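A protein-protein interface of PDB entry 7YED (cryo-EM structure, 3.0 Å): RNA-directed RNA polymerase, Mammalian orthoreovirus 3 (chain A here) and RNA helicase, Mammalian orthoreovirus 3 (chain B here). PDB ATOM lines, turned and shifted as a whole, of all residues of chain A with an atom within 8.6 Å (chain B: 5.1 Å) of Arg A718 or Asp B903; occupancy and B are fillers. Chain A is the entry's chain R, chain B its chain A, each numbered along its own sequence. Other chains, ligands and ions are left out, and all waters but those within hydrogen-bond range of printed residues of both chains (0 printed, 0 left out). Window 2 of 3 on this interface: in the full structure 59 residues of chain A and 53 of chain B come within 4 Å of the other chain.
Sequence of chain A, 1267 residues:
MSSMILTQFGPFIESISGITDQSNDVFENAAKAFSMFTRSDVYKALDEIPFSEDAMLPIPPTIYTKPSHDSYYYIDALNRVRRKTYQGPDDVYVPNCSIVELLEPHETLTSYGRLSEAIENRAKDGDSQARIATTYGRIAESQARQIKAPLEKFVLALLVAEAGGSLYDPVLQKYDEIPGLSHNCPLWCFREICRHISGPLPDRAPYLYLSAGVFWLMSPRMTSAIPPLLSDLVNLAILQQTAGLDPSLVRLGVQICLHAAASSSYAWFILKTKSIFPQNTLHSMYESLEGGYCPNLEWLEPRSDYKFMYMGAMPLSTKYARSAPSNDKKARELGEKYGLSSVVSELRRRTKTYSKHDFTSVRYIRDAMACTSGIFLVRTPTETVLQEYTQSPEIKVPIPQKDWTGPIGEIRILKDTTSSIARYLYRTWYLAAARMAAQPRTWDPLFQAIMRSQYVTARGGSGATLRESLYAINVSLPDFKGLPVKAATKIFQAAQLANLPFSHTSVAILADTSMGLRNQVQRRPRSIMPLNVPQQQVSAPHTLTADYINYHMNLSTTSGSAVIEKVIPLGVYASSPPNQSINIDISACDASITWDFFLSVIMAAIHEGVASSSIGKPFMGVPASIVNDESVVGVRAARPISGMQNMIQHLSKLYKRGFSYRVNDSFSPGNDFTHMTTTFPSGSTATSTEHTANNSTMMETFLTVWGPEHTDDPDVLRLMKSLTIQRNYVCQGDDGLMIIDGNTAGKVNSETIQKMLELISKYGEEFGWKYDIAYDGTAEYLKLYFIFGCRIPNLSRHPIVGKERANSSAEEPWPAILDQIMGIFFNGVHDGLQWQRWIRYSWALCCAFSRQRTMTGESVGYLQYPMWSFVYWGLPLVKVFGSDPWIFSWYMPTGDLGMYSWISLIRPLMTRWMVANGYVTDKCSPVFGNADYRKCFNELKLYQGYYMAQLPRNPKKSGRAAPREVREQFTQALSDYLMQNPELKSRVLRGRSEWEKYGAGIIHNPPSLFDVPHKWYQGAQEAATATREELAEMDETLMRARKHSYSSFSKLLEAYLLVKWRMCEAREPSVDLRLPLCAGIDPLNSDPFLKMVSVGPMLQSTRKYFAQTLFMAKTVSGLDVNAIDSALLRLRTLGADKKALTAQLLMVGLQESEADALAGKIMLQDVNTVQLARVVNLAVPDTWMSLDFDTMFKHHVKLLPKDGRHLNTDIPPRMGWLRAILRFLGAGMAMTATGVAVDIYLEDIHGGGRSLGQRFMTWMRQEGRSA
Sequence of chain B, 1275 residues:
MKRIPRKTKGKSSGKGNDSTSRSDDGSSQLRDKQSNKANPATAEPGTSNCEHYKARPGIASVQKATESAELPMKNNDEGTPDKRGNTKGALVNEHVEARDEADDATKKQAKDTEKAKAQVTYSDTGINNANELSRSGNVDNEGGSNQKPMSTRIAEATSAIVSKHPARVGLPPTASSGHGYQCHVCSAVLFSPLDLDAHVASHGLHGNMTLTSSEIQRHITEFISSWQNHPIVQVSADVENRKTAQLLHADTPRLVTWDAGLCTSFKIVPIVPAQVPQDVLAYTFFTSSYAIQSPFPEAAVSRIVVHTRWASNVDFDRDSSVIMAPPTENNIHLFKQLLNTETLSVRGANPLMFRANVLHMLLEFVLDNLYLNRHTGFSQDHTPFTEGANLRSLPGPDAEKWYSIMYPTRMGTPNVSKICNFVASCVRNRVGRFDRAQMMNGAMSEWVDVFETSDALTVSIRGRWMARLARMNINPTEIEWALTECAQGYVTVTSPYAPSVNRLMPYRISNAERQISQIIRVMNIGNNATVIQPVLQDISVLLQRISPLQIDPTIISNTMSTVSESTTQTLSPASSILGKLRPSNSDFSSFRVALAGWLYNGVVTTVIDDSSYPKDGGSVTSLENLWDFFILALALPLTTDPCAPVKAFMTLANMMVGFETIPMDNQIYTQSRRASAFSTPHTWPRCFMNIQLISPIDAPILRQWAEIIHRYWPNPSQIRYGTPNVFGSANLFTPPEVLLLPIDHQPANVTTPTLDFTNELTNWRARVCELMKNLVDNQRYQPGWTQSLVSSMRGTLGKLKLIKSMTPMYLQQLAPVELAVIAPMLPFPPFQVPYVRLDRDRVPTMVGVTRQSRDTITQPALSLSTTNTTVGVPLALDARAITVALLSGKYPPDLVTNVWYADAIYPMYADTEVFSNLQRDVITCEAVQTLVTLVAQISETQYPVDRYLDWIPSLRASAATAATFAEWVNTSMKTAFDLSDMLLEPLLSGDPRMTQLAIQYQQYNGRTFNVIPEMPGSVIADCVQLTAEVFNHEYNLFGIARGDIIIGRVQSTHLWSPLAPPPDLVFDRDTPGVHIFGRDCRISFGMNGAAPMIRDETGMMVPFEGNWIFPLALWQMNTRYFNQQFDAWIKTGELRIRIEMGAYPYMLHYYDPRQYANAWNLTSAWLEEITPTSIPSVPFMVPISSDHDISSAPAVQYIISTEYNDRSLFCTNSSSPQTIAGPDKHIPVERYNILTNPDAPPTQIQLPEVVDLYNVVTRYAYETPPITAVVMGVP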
ATOM      1  N   PRO A 708     -15.132   3.343 -22.566  1.00  0.00           N
ATOM      2  CA  PRO A 708     -14.083   3.544 -21.552  1.00  0.00           C
ATOM      3  C   PRO A 708     -13.794   2.328 -20.686  1.00  0.00           C
ATOM      4  O   PRO A 708     -12.771   2.328 -19.991  1.00  0.00           O
ATOM      5  CB  PRO A 708     -14.630   4.701 -20.707  1.00  0.00           C
ATOM      6  CG  PRO A 708     -15.561   5.416 -21.610  1.00  0.00           C
ATOM      7  CD  PRO A 708     -16.196   4.353 -22.451  1.00  0.00           C
ATOM      8  N   THR A 711     -11.098  -0.223 -23.247  1.00  0.00           N
ATOM      9  CA  THR A 711      -9.912   0.258 -23.938  1.00  0.00           C
ATOM     10  C   THR A 711      -8.990   0.931 -22.935  1.00  0.00           C
ATOM     11  O   THR A 711      -9.445   1.530 -21.958  1.00  0.00           O
ATOM     12  CB  THR A 711     -10.251   1.241 -25.052  1.00  0.00           C
ATOM     13  OG1 THR A 711      -9.068   1.526 -25.808  1.00  0.00           O
ATOM     14  CG2 THR A 711     -10.768   2.525 -24.460  1.00  0.00           C
ATOM     15  N   ASP A 712      -7.691   0.839 -23.190  1.00  0.00           N
ATOM     16  CA  ASP A 712      -6.699   1.275 -22.220  1.00  0.00           C
ATOM     17  C   ASP A 712      -5.836   2.440 -22.676  1.00  0.00           C
ATOM     18  O   ASP A 712      -5.382   3.210 -21.827  1.00  0.00           O
ATOM     19  CB  ASP A 712      -5.781   0.106 -21.839  1.00  0.00           C
ATOM     20  CG  ASP A 712      -4.841   0.453 -20.708  1.00  0.00           C
ATOM     21  OD1 ASP A 712      -5.310   0.542 -19.553  1.00  0.00           O
ATOM     22  OD2 ASP A 712      -3.635   0.633 -20.972  1.00  0.00           O
ATOM     23  N   ASP A 713      -5.590   2.595 -23.972  1.00  0.00           N
ATOM     24  CA  ASP A 713      -4.698   3.657 -24.412  1.00  0.00           C
ATOM     25  C   ASP A 713      -5.341   5.024 -24.180  1.00  0.00           C
ATOM     26  O   ASP A 713      -6.557   5.174 -24.310  1.00  0.00           O
ATOM     27  CB  ASP A 713      -4.324   3.489 -25.882  1.00  0.00           C
ATOM     28  CG  ASP A 713      -5.522   3.500 -26.800  1.00  0.00           C
ATOM     29  OD1 ASP A 713      -6.667   3.512 -26.312  1.00  0.00           O
ATOM     30  OD2 ASP A 713      -5.313   3.505 -28.029  1.00  0.00           O
ATOM     31  N   PRO A 714      -4.552   6.031 -23.815  1.00  0.00           N
ATOM     32  CA  PRO A 714      -5.133   7.353 -23.535  1.00  0.00           C
ATOM     33  C   PRO A 714      -5.786   8.000 -24.740  1.00  0.00           C
ATOM     34  O   PRO A 714      -6.726   8.789 -24.578  1.00  0.00           O
ATOM     35  CB  PRO A 714      -3.923   8.163 -23.052  1.00  0.00           C
ATOM     36  CG  PRO A 714      -2.953   7.138 -22.559  1.00  0.00           C
ATOM     37  CD  PRO A 714      -3.126   5.961 -23.463  1.00  0.00           C
ATOM     38  N   ASP A 715      -5.316   7.692 -25.947  1.00  0.00           N
ATOM     39  CA  ASP A 715      -5.834   8.355 -27.138  1.00  0.00           C
ATOM     40  C   ASP A 715      -7.289   7.985 -27.388  1.00  0.00           C
ATOM     41  O   ASP A 715      -8.134   8.861 -27.609  1.00  0.00           O
ATOM     42  CB  ASP A 715      -4.973   7.995 -28.345  1.00  0.00           C
ATOM     43  CG  ASP A 715      -3.590   8.595 -28.265  1.00  0.00           C
ATOM     44  OD1 ASP A 715      -3.446   9.673 -27.653  1.00  0.00           O
ATOM     45  OD2 ASP A 715      -2.643   7.989 -28.808  1.00  0.00           O
ATOM     46  N   VAL A 716      -7.604   6.691 -27.363  1.00  0.00           N
ATOM     47  CA  VAL A 716      -8.973   6.266 -27.629  1.00  0.00           C
ATOM     48  C   VAL A 716      -9.903   6.746 -26.524  1.00  0.00           C
ATOM     49  O   VAL A 716     -11.058   7.101 -26.779  1.00  0.00           O
ATOM     50  CB  VAL A 716      -9.037   4.742 -27.802  1.00  0.00           C
ATOM     51  CG1 VAL A 716     -10.469   4.305 -28.013  1.00  0.00           C
ATOM     52  CG2 VAL A 716      -8.174   4.313 -28.965  1.00  0.00           C
ATOM     53  N   LEU A 717      -9.417   6.772 -25.282  1.00  0.00           N
ATOM     54  CA  LEU A 717     -10.230   7.294 -24.191  1.00  0.00           C
ATOM     55  C   LEU A 717     -10.536   8.770 -24.393  1.00  0.00           C
ATOM     56  O   LEU A 717     -11.682   9.204 -24.227  1.00  0.00           O
ATOM     57  CB  LEU A 717      -9.526   7.070 -22.857  1.00  0.00           C
ATOM     58  CG  LEU A 717      -9.390   5.612 -22.429  1.00  0.00           C
ATOM     59  CD1 LEU A 717      -8.549   5.485 -21.172  1.00  0.00           C
ATOM     60  CD2 LEU A 717     -10.764   5.018 -22.212  1.00  0.00           C
ATOM     61  N   ARG A 718      -9.527   9.560 -24.764  1.00  0.00           N
ATOM     62  CA  ARG A 718      -9.772  10.980 -24.983  1.00  0.00           C
ATOM     63  C   ARG A 718     -10.644  11.216 -26.206  1.00  0.00           C
ATOM     64  O   ARG A 718     -11.324  12.245 -26.288  1.00  0.00           O
ATOM     65  CB  ARG A 718      -8.455  11.735 -25.126  1.00  0.00           C
ATOM     66  CG  ARG A 718      -8.656  13.224 -25.273  1.00  0.00           C
ATOM     67  CD  ARG A 718      -7.353  13.979 -25.377  1.00  0.00           C
ATOM     68  NE  ARG A 718      -7.599  15.411 -25.485  1.00  0.00           N
ATOM     69  CZ  ARG A 718      -7.811  16.039 -26.634  1.00  0.00           C
ATOM     70  NH1 ARG A 718      -7.801  15.356 -27.768  1.00  0.00           N
ATOM     71  NH2 ARG A 718      -8.033  17.344 -26.650  1.00  0.00           N
ATOM     72  N   LEU A 719     -10.636  10.294 -27.165  1.00  0.00           N
ATOM     73  CA  LEU A 719     -11.516  10.452 -28.317  1.00  0.00           C
ATOM     74  C   LEU A 719     -12.955  10.096 -27.970  1.00  0.00           C
ATOM     75  O   LEU A 719     -13.889  10.743 -28.454  1.00  0.00           O
ATOM     76  CB  LEU A 719     -11.026   9.597 -29.483  1.00  0.00           C
ATOM     77  CG  LEU A 719     -11.838   9.744 -30.769  1.00  0.00           C
ATOM     78  CD1 LEU A 719     -11.762  11.166 -31.279  1.00  0.00           C
ATOM     79  CD2 LEU A 719     -11.348   8.776 -31.822  1.00  0.00           C
ATOM     80  N   MET A 720     -13.159   9.076 -27.139  1.00  0.00           N
ATOM     81  CA  MET A 720     -14.512   8.697 -26.761  1.00  0.00           C
ATOM     82  C   MET A 720     -15.096   9.597 -25.685  1.00  0.00           C
ATOM     83  O   MET A 720     -16.315   9.592 -25.492  1.00  0.00           O
ATOM     84  CB  MET A 720     -14.551   7.250 -26.283  1.00  0.00           C
ATOM     85  CG  MET A 720     -14.272   6.236 -27.361  1.00  0.00           C
ATOM     86  SD  MET A 720     -14.440   4.574 -26.716  1.00  0.00           S
ATOM     87  CE  MET A 720     -12.983   4.507 -25.693  1.00  0.00           C
ATOM     88  N   LYS A 721     -14.270  10.357 -24.972  1.00  0.00           N
ATOM     89  CA  LYS A 721     -14.801  11.292 -23.990  1.00  0.00           C
ATOM     90  C   LYS A 721     -15.200  12.627 -24.596  1.00  0.00           C
ATOM     91  O   LYS A 721     -16.051  13.317 -24.027  1.00  0.00           O
ATOM     92  CB  LYS A 721     -13.784  11.532 -22.874  1.00  0.00           C
ATOM     93  CG  LYS A 721     -13.544  10.323 -21.999  1.00  0.00           C
ATOM     94  CD  LYS A 721     -12.616  10.653 -20.850  1.00  0.00           C
ATOM     95  CE  LYS A 721     -12.317   9.413 -20.031  1.00  0.00           C
ATOM     96  NZ  LYS A 721     -13.535   8.915 -19.345  1.00  0.00           N
ATOM     97  N   SER A 722     -14.622  13.002 -25.731  1.00  0.00           N
ATOM     98  CA  SER A 722     -14.953  14.260 -26.382  1.00  0.00           C
ATOM     99  C   SER A 722     -16.118  14.138 -27.352  1.00  0.00           C
ATOM    100  O   SER A 722     -16.455  15.122 -28.017  1.00  0.00           O
ATOM    101  CB  SER A 722     -13.730  14.808 -27.122  1.00  0.00           C
ATOM    102  OG  SER A 722     -13.372  13.969 -28.202  1.00  0.00           O
ATOM    103  N   LEU A 723     -16.738  12.967 -27.449  1.00  0.00           N
ATOM    104  CA  LEU A 723     -17.836  12.733 -28.371  1.00  0.00           C
ATOM    105  C   LEU A 723     -19.135  12.543 -27.603  1.00  0.00           C
ATOM    106  O   LEU A 723     -19.162  11.880 -26.564  1.00  0.00           O
ATOM    107  CB  LEU A 723     -17.571  11.502 -29.238  1.00  0.00           C
ATOM    108  CG  LEU A 723     -16.419  11.585 -30.233  1.00  0.00           C
ATOM    109  CD1 LEU A 723     -16.199  10.240 -30.886  1.00  0.00           C
ATOM    110  CD2 LEU A 723     -16.723  12.628 -31.275  1.00  0.00           C
ATOM    111  N   ASP A 741     -14.802  16.020 -35.318  1.00  0.00           N
ATOM    112  CA  ASP A 741     -14.229  17.331 -35.567  1.00  0.00           C
ATOM    113  C   ASP A 741     -12.710  17.268 -35.571  1.00  0.00           C
ATOM    114  O   ASP A 741     -12.100  16.387 -34.959  1.00  0.00           O
ATOM    115  CB  ASP A 741     -14.701  18.325 -34.509  1.00  0.00           C
ATOM    116  CG  ASP A 741     -16.177  18.637 -34.619  1.00  0.00           C
ATOM    117  OD1 ASP A 741     -16.707  18.590 -35.748  1.00  0.00           O
ATOM    118  OD2 ASP A 741     -16.809  18.924 -33.583  1.00  0.00           O
ATOM    119  N   ASN A 743      -9.195  18.805 -34.440  1.00  0.00           N
ATOM    120  CA  ASN A 743      -8.640  19.596 -33.354  1.00  0.00           C
ATOM    121  C   ASN A 743      -7.695  20.643 -33.939  1.00  0.00           C
ATOM    122  O   ASN A 743      -7.674  20.890 -35.146  1.00  0.00           O
ATOM    123  CB  ASN A 743      -7.977  18.682 -32.328  1.00  0.00           C
ATOM    124  CG  ASN A 743      -6.884  17.822 -32.923  1.00  0.00           C
ATOM    125  OD1 ASN A 743      -6.479  18.005 -34.066  1.00  0.00           O
ATOM    126  ND2 ASN A 743      -6.418  16.854 -32.149  1.00  0.00           N
ATOM    127  N   THR A 744      -6.908  21.290 -33.084  1.00  0.00           N
ATOM    128  CA  THR A 744      -6.014  22.327 -33.579  1.00  0.00           C
ATOM    129  C   THR A 744      -4.803  21.751 -34.296  1.00  0.00           C
ATOM    130  O   THR A 744      -4.264  22.395 -35.201  1.00  0.00           O
ATOM    131  CB  THR A 744      -5.544  23.219 -32.439  1.00  0.00           C
ATOM    132  OG1 THR A 744      -6.679  23.792 -31.783  1.00  0.00           O
ATOM    133  CG2 THR A 744      -4.693  24.331 -32.993  1.00  0.00           C
ATOM    134  N   ALA A 745      -4.358  20.556 -33.913  1.00  0.00           N
ATOM    135  CA  ALA A 745      -3.226  19.930 -34.583  1.00  0.00           C
ATOM    136  C   ALA A 745      -3.555  19.452 -35.991  1.00  0.00           C
ATOM    137  O   ALA A 745      -2.648  18.989 -36.690  1.00  0.00           O
ATOM    138  CB  ALA A 745      -2.706  18.759 -33.750  1.00  0.00           C
ATOM    139  N   VAL A 748      -7.832  14.588 -36.908  1.00  0.00           N
ATOM    140  CA  VAL A 748      -7.629  13.652 -35.814  1.00  0.00           C
ATOM    141  C   VAL A 748      -6.874  12.434 -36.337  1.00  0.00           C
ATOM    142  O   VAL A 748      -7.008  12.047 -37.503  1.00  0.00           O
ATOM    143  CB  VAL A 748      -8.974  13.248 -35.185  1.00  0.00           C
ATOM    144  CG1 VAL A 748      -8.772  12.217 -34.093  1.00  0.00           C
ATOM    145  CG2 VAL A 748      -9.686  14.466 -34.635  1.00  0.00           C
ATOM    146  N   THR A 752      -6.200   5.878 -33.965  1.00  0.00           N
ATOM    147  CA  THR A 752      -7.160   5.959 -32.871  1.00  0.00           C
ATOM    148  C   THR A 752      -8.584   5.793 -33.382  1.00  0.00           C
ATOM    149  O   THR A 752      -9.385   5.065 -32.785  1.00  0.00           O
ATOM    150  CB  THR A 752      -7.013   7.292 -32.145  1.00  0.00           C
ATOM    151  OG1 THR A 752      -7.319   8.361 -33.052  1.00  0.00           O
ATOM    152  CG2 THR A 752      -5.592   7.466 -31.654  1.00  0.00           C
ATOM    153  N   MET A 756     -11.212   2.775 -32.364  1.00  0.00           N
ATOM    154  CA  MET A 756     -12.588   3.023 -31.947  1.00  0.00           C
ATOM    155  C   MET A 756     -13.571   2.284 -32.848  1.00  0.00           C
ATOM    156  O   MET A 756     -14.598   1.775 -32.383  1.00  0.00           O
ATOM    157  CB  MET A 756     -12.884   4.523 -31.947  1.00  0.00           C
ATOM    158  CG  MET A 756     -14.245   4.872 -31.417  1.00  0.00           C
ATOM    159  SD  MET A 756     -14.569   6.640 -31.418  1.00  0.00           S
ATOM    160  CE  MET A 756     -14.752   6.935 -33.171  1.00  0.00           C
ATOM    161  N   VAL B 899     -12.469  24.769 -18.748  1.00  0.00           N
ATOM    162  CA  VAL B 899     -12.734  23.468 -19.346  1.00  0.00           C
ATOM    163  C   VAL B 899     -12.626  23.545 -20.860  1.00  0.00           C
ATOM    164  O   VAL B 899     -12.158  22.602 -21.509  1.00  0.00           O
ATOM    165  CB  VAL B 899     -14.109  22.947 -18.904  1.00  0.00           C
ATOM    166  CG1 VAL B 899     -14.424  21.647 -19.605  1.00  0.00           C
ATOM    167  CG2 VAL B 899     -14.136  22.754 -17.411  1.00  0.00           C
ATOM    168  N   TRP B 900     -13.055  24.660 -21.452  1.00  0.00           N
ATOM    169  CA  TRP B 900     -12.942  24.812 -22.897  1.00  0.00           C
ATOM    170  C   TRP B 900     -11.485  24.813 -23.332  1.00  0.00           C
ATOM    171  O   TRP B 900     -11.075  24.024 -24.191  1.00  0.00           O
ATOM    172  CB  TRP B 900     -13.629  26.098 -23.352  1.00  0.00           C
ATOM    173  CG  TRP B 900     -13.592  26.290 -24.832  1.00  0.00           C
ATOM    174  CD1 TRP B 900     -12.734  27.078 -25.531  1.00  0.00           C
ATOM    175  CD2 TRP B 900     -14.461  25.690 -25.796  1.00  0.00           C
ATOM    176  NE1 TRP B 900     -13.006  27.002 -26.871  1.00  0.00           N
ATOM    177  CE2 TRP B 900     -14.065  26.157 -27.060  1.00  0.00           C
ATOM    178  CE3 TRP B 900     -15.534  24.802 -25.713  1.00  0.00           C
ATOM    179  CZ2 TRP B 900     -14.701  25.767 -28.229  1.00  0.00           C
ATOM    180  CZ3 TRP B 900     -16.163  24.417 -26.873  1.00  0.00           C
ATOM    181  CH2 TRP B 900     -15.746  24.898 -28.115  1.00  0.00           C
ATOM    182  N   TYR B 901     -10.684  25.703 -22.749  1.00  0.00           N
ATOM    183  CA  TYR B 901      -9.308  25.817 -23.214  1.00  0.00           C
ATOM    184  C   TYR B 901      -8.477  24.600 -22.843  1.00  0.00           C
ATOM    185  O   TYR B 901      -7.548  24.255 -23.578  1.00  0.00           O
ATOM    186  CB  TYR B 901      -8.661  27.089 -22.679  1.00  0.00           C
ATOM    187  CG  TYR B 901      -9.221  28.342 -23.295  1.00  0.00           C
ATOM    188  CD1 TYR B 901      -8.833  28.745 -24.558  1.00  0.00           C
ATOM    189  CD2 TYR B 901     -10.133  29.123 -22.615  1.00  0.00           C
ATOM    190  CE1 TYR B 901      -9.341  29.883 -25.125  1.00  0.00           C
ATOM    191  CE2 TYR B 901     -10.646  30.262 -23.175  1.00  0.00           C
ATOM    192  CZ  TYR B 901     -10.245  30.637 -24.431  1.00  0.00           C
ATOM    193  OH  TYR B 901     -10.749  31.778 -25.005  1.00  0.00           O
ATOM    194  N   ALA B 902      -8.811  23.913 -21.745  1.00  0.00           N
ATOM    195  CA  ALA B 902      -7.992  22.794 -21.295  1.00  0.00           C
ATOM    196  C   ALA B 902      -7.915  21.682 -22.330  1.00  0.00           C
ATOM    197  O   ALA B 902      -6.906  20.973 -22.399  1.00  0.00           O
ATOM    198  CB  ALA B 902      -8.534  22.247 -19.978  1.00  0.00           C
ATOM    199  N   ASP B 903      -8.957  21.507 -23.137  1.00  0.00           N
ATOM    200  CA  ASP B 903      -8.915  20.517 -24.198  1.00  0.00           C
ATOM    201  C   ASP B 903      -8.904  21.122 -25.591  1.00  0.00           C
ATOM    202  O   ASP B 903      -8.726  20.382 -26.561  1.00  0.00           O
ATOM    203  CB  ASP B 903     -10.086  19.532 -24.073  1.00  0.00           C
ATOM    204  CG  ASP B 903     -11.434  20.195 -24.214  1.00  0.00           C
ATOM    205  OD1 ASP B 903     -11.490  21.430 -24.352  1.00  0.00           O
ATOM    206  OD2 ASP B 903     -12.450  19.471 -24.189  1.00  0.00           O
ATOM    207  N   ALA B 904      -9.092  22.434 -25.724  1.00  0.00           N
ATOM    208  CA  ALA B 904      -8.841  23.044 -27.022  1.00  0.00           C
ATOM    209  C   ALA B 904      -7.349  23.222 -27.271  1.00  0.00           C
ATOM    210  O   ALA B 904      -6.888  23.086 -28.408  1.00  0.00           O
ATOM    211  CB  ALA B 904      -9.567  24.384 -27.123  1.00  0.00           C
ATOM    212  N   ILE B 905      -6.580  23.501 -26.219  1.00  0.00           N
ATOM    213  CA  ILE B 905      -5.163  23.811 -26.359  1.00  0.00           C
ATOM    214  C   ILE B 905      -4.276  22.573 -26.304  1.00  0.00           C
ATOM    215  O   ILE B 905      -3.117  22.631 -26.738  1.00  0.00           O
ATOM    216  CB  ILE B 905      -4.770  24.821 -25.265  1.00  0.00           C
ATOM    217  CG1 ILE B 905      -5.535  26.128 -25.461  1.00  0.00           C
ATOM    218  CG2 ILE B 905      -3.291  25.090 -25.256  1.00  0.00           C
ATOM    219  CD1 ILE B 905      -5.412  27.089 -24.305  1.00  0.00           C
ATOM    220  N   TYR B 906      -4.791  21.453 -25.811  1.00  0.00           N
ATOM    221  CA  TYR B 906      -3.958  20.266 -25.622  1.00  0.00           C
ATOM    222  C   TYR B 906      -3.367  19.716 -26.911  1.00  0.00           C
ATOM    223  O   TYR B 906      -2.148  19.478 -26.948  1.00  0.00           O
ATOM    224  CB  TYR B 906      -4.766  19.184 -24.906  1.00  0.00           C
ATOM    225  CG  TYR B 906      -3.974  17.929 -24.654  1.00  0.00           C
ATOM    226  CD1 TYR B 906      -3.041  17.872 -23.636  1.00  0.00           C
ATOM    227  CD2 TYR B 906      -4.149  16.807 -25.444  1.00  0.00           C
ATOM    228  CE1 TYR B 906      -2.312  16.730 -23.405  1.00  0.00           C
ATOM    229  CE2 TYR B 906      -3.423  15.662 -25.222  1.00  0.00           C
ATOM    230  CZ  TYR B 906      -2.508  15.628 -24.201  1.00  0.00           C
ATOM    231  OH  TYR B 906      -1.783  14.484 -23.979  1.00  0.00           O
ATOM    232  N   PRO B 907      -4.136  19.470 -27.974  1.00  0.00           N
ATOM    233  CA  PRO B 907      -3.576  18.745 -29.125  1.00  0.00           C
ATOM    234  C   PRO B 907      -2.435  19.455 -29.829  1.00  0.00           C
ATOM    235  O   PRO B 907      -1.707  18.798 -30.581  1.00  0.00           O
ATOM    236  CB  PRO B 907      -4.782  18.585 -30.055  1.00  0.00           C
ATOM    237  CG  PRO B 907      -5.950  18.663 -29.166  1.00  0.00           C
ATOM    238  CD  PRO B 907      -5.588  19.655 -28.117  1.00  0.00           C
ATOM    239  N   PRO B1275      -4.072  14.265 -20.393  1.00  0.00           N
ATOM    240  CA  PRO B1275      -5.225  14.662 -21.207  1.00  0.00           C
ATOM    241  C   PRO B1275      -6.389  15.180 -20.372  1.00  0.00           C
ATOM    242  O   PRO B1275      -6.401  14.953 -19.163  1.00  0.00           O
ATOM    243  CB  PRO B1275      -5.609  13.365 -21.922  1.00  0.00           C
ATOM    244  CG  PRO B1275      -4.362  12.559 -21.934  1.00  0.00           C
ATOM    245  CD  PRO B1275      -3.684  12.868 -20.637  1.00  0.00           C
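The side-chain hydroxyl (OG1) of Thr A744 lies within hydrogen-bond range of the backbone carbonyl oxygen (O) of Ala B904, at 3.5 Å. The backbone carbonyl oxygen (O) of Asp B903 lies within hydrogen-bond range of the guanidinium group (NH2) of Arg A718 (3.1 Å).
The side-chain carboxylate of Asp B903 lies close to the backbone carbonyl oxygen of Trp B900, at 2.6 Å. OD1 of Asn A743 lies within hydrogen-bond range of N of Ala A745 (3.3 Å). O of Arg A718 sits at hydrogen-bond distance from OG of Ser A722 (3.3 Å).
Among the printed residues, merely in contact across the chains: Asn A743 with Pro B907 (3.2 Å), Ala A745 with Pro B907 (3.3 Å), Arg A718 with Pro B907 (3.5 Å), Arg A718 with Tyr B906 (3.7 Å) and Arg A718 with Pro B1275 (3.9 Å).
Arg A718 touches four residues of chain B. Of the printed residues of chain A, Asp B903 touches Arg A718 (3.1 Å). No residue of chain A comes within 4 Å of Ala B902. Of the printed residues of chain B, Thr A744 touches Ala B904. Of the printed residues of chain B, Asn A743 touches Pro B907. Asp A712 touches none of the printed residues of chain B. Leu A719 touches none of the printed residues of chain B. The nearest printed residue of chain A that does not touch Pro B907 is Thr A744 (4.6 Å).
Of the 21 printed residues of chain A, 4 touch a printed residue of chain B. Hydrophobic or aromatic side chains of chain A that line the printed part of chain B: Ala A745. Among the printed residues, 7 pairs touch across the chains. Among the printed residues, no Asp or Glu carboxylate lies within 4 Å of a Lys or Arg side-chain nitrogen of the other chain.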
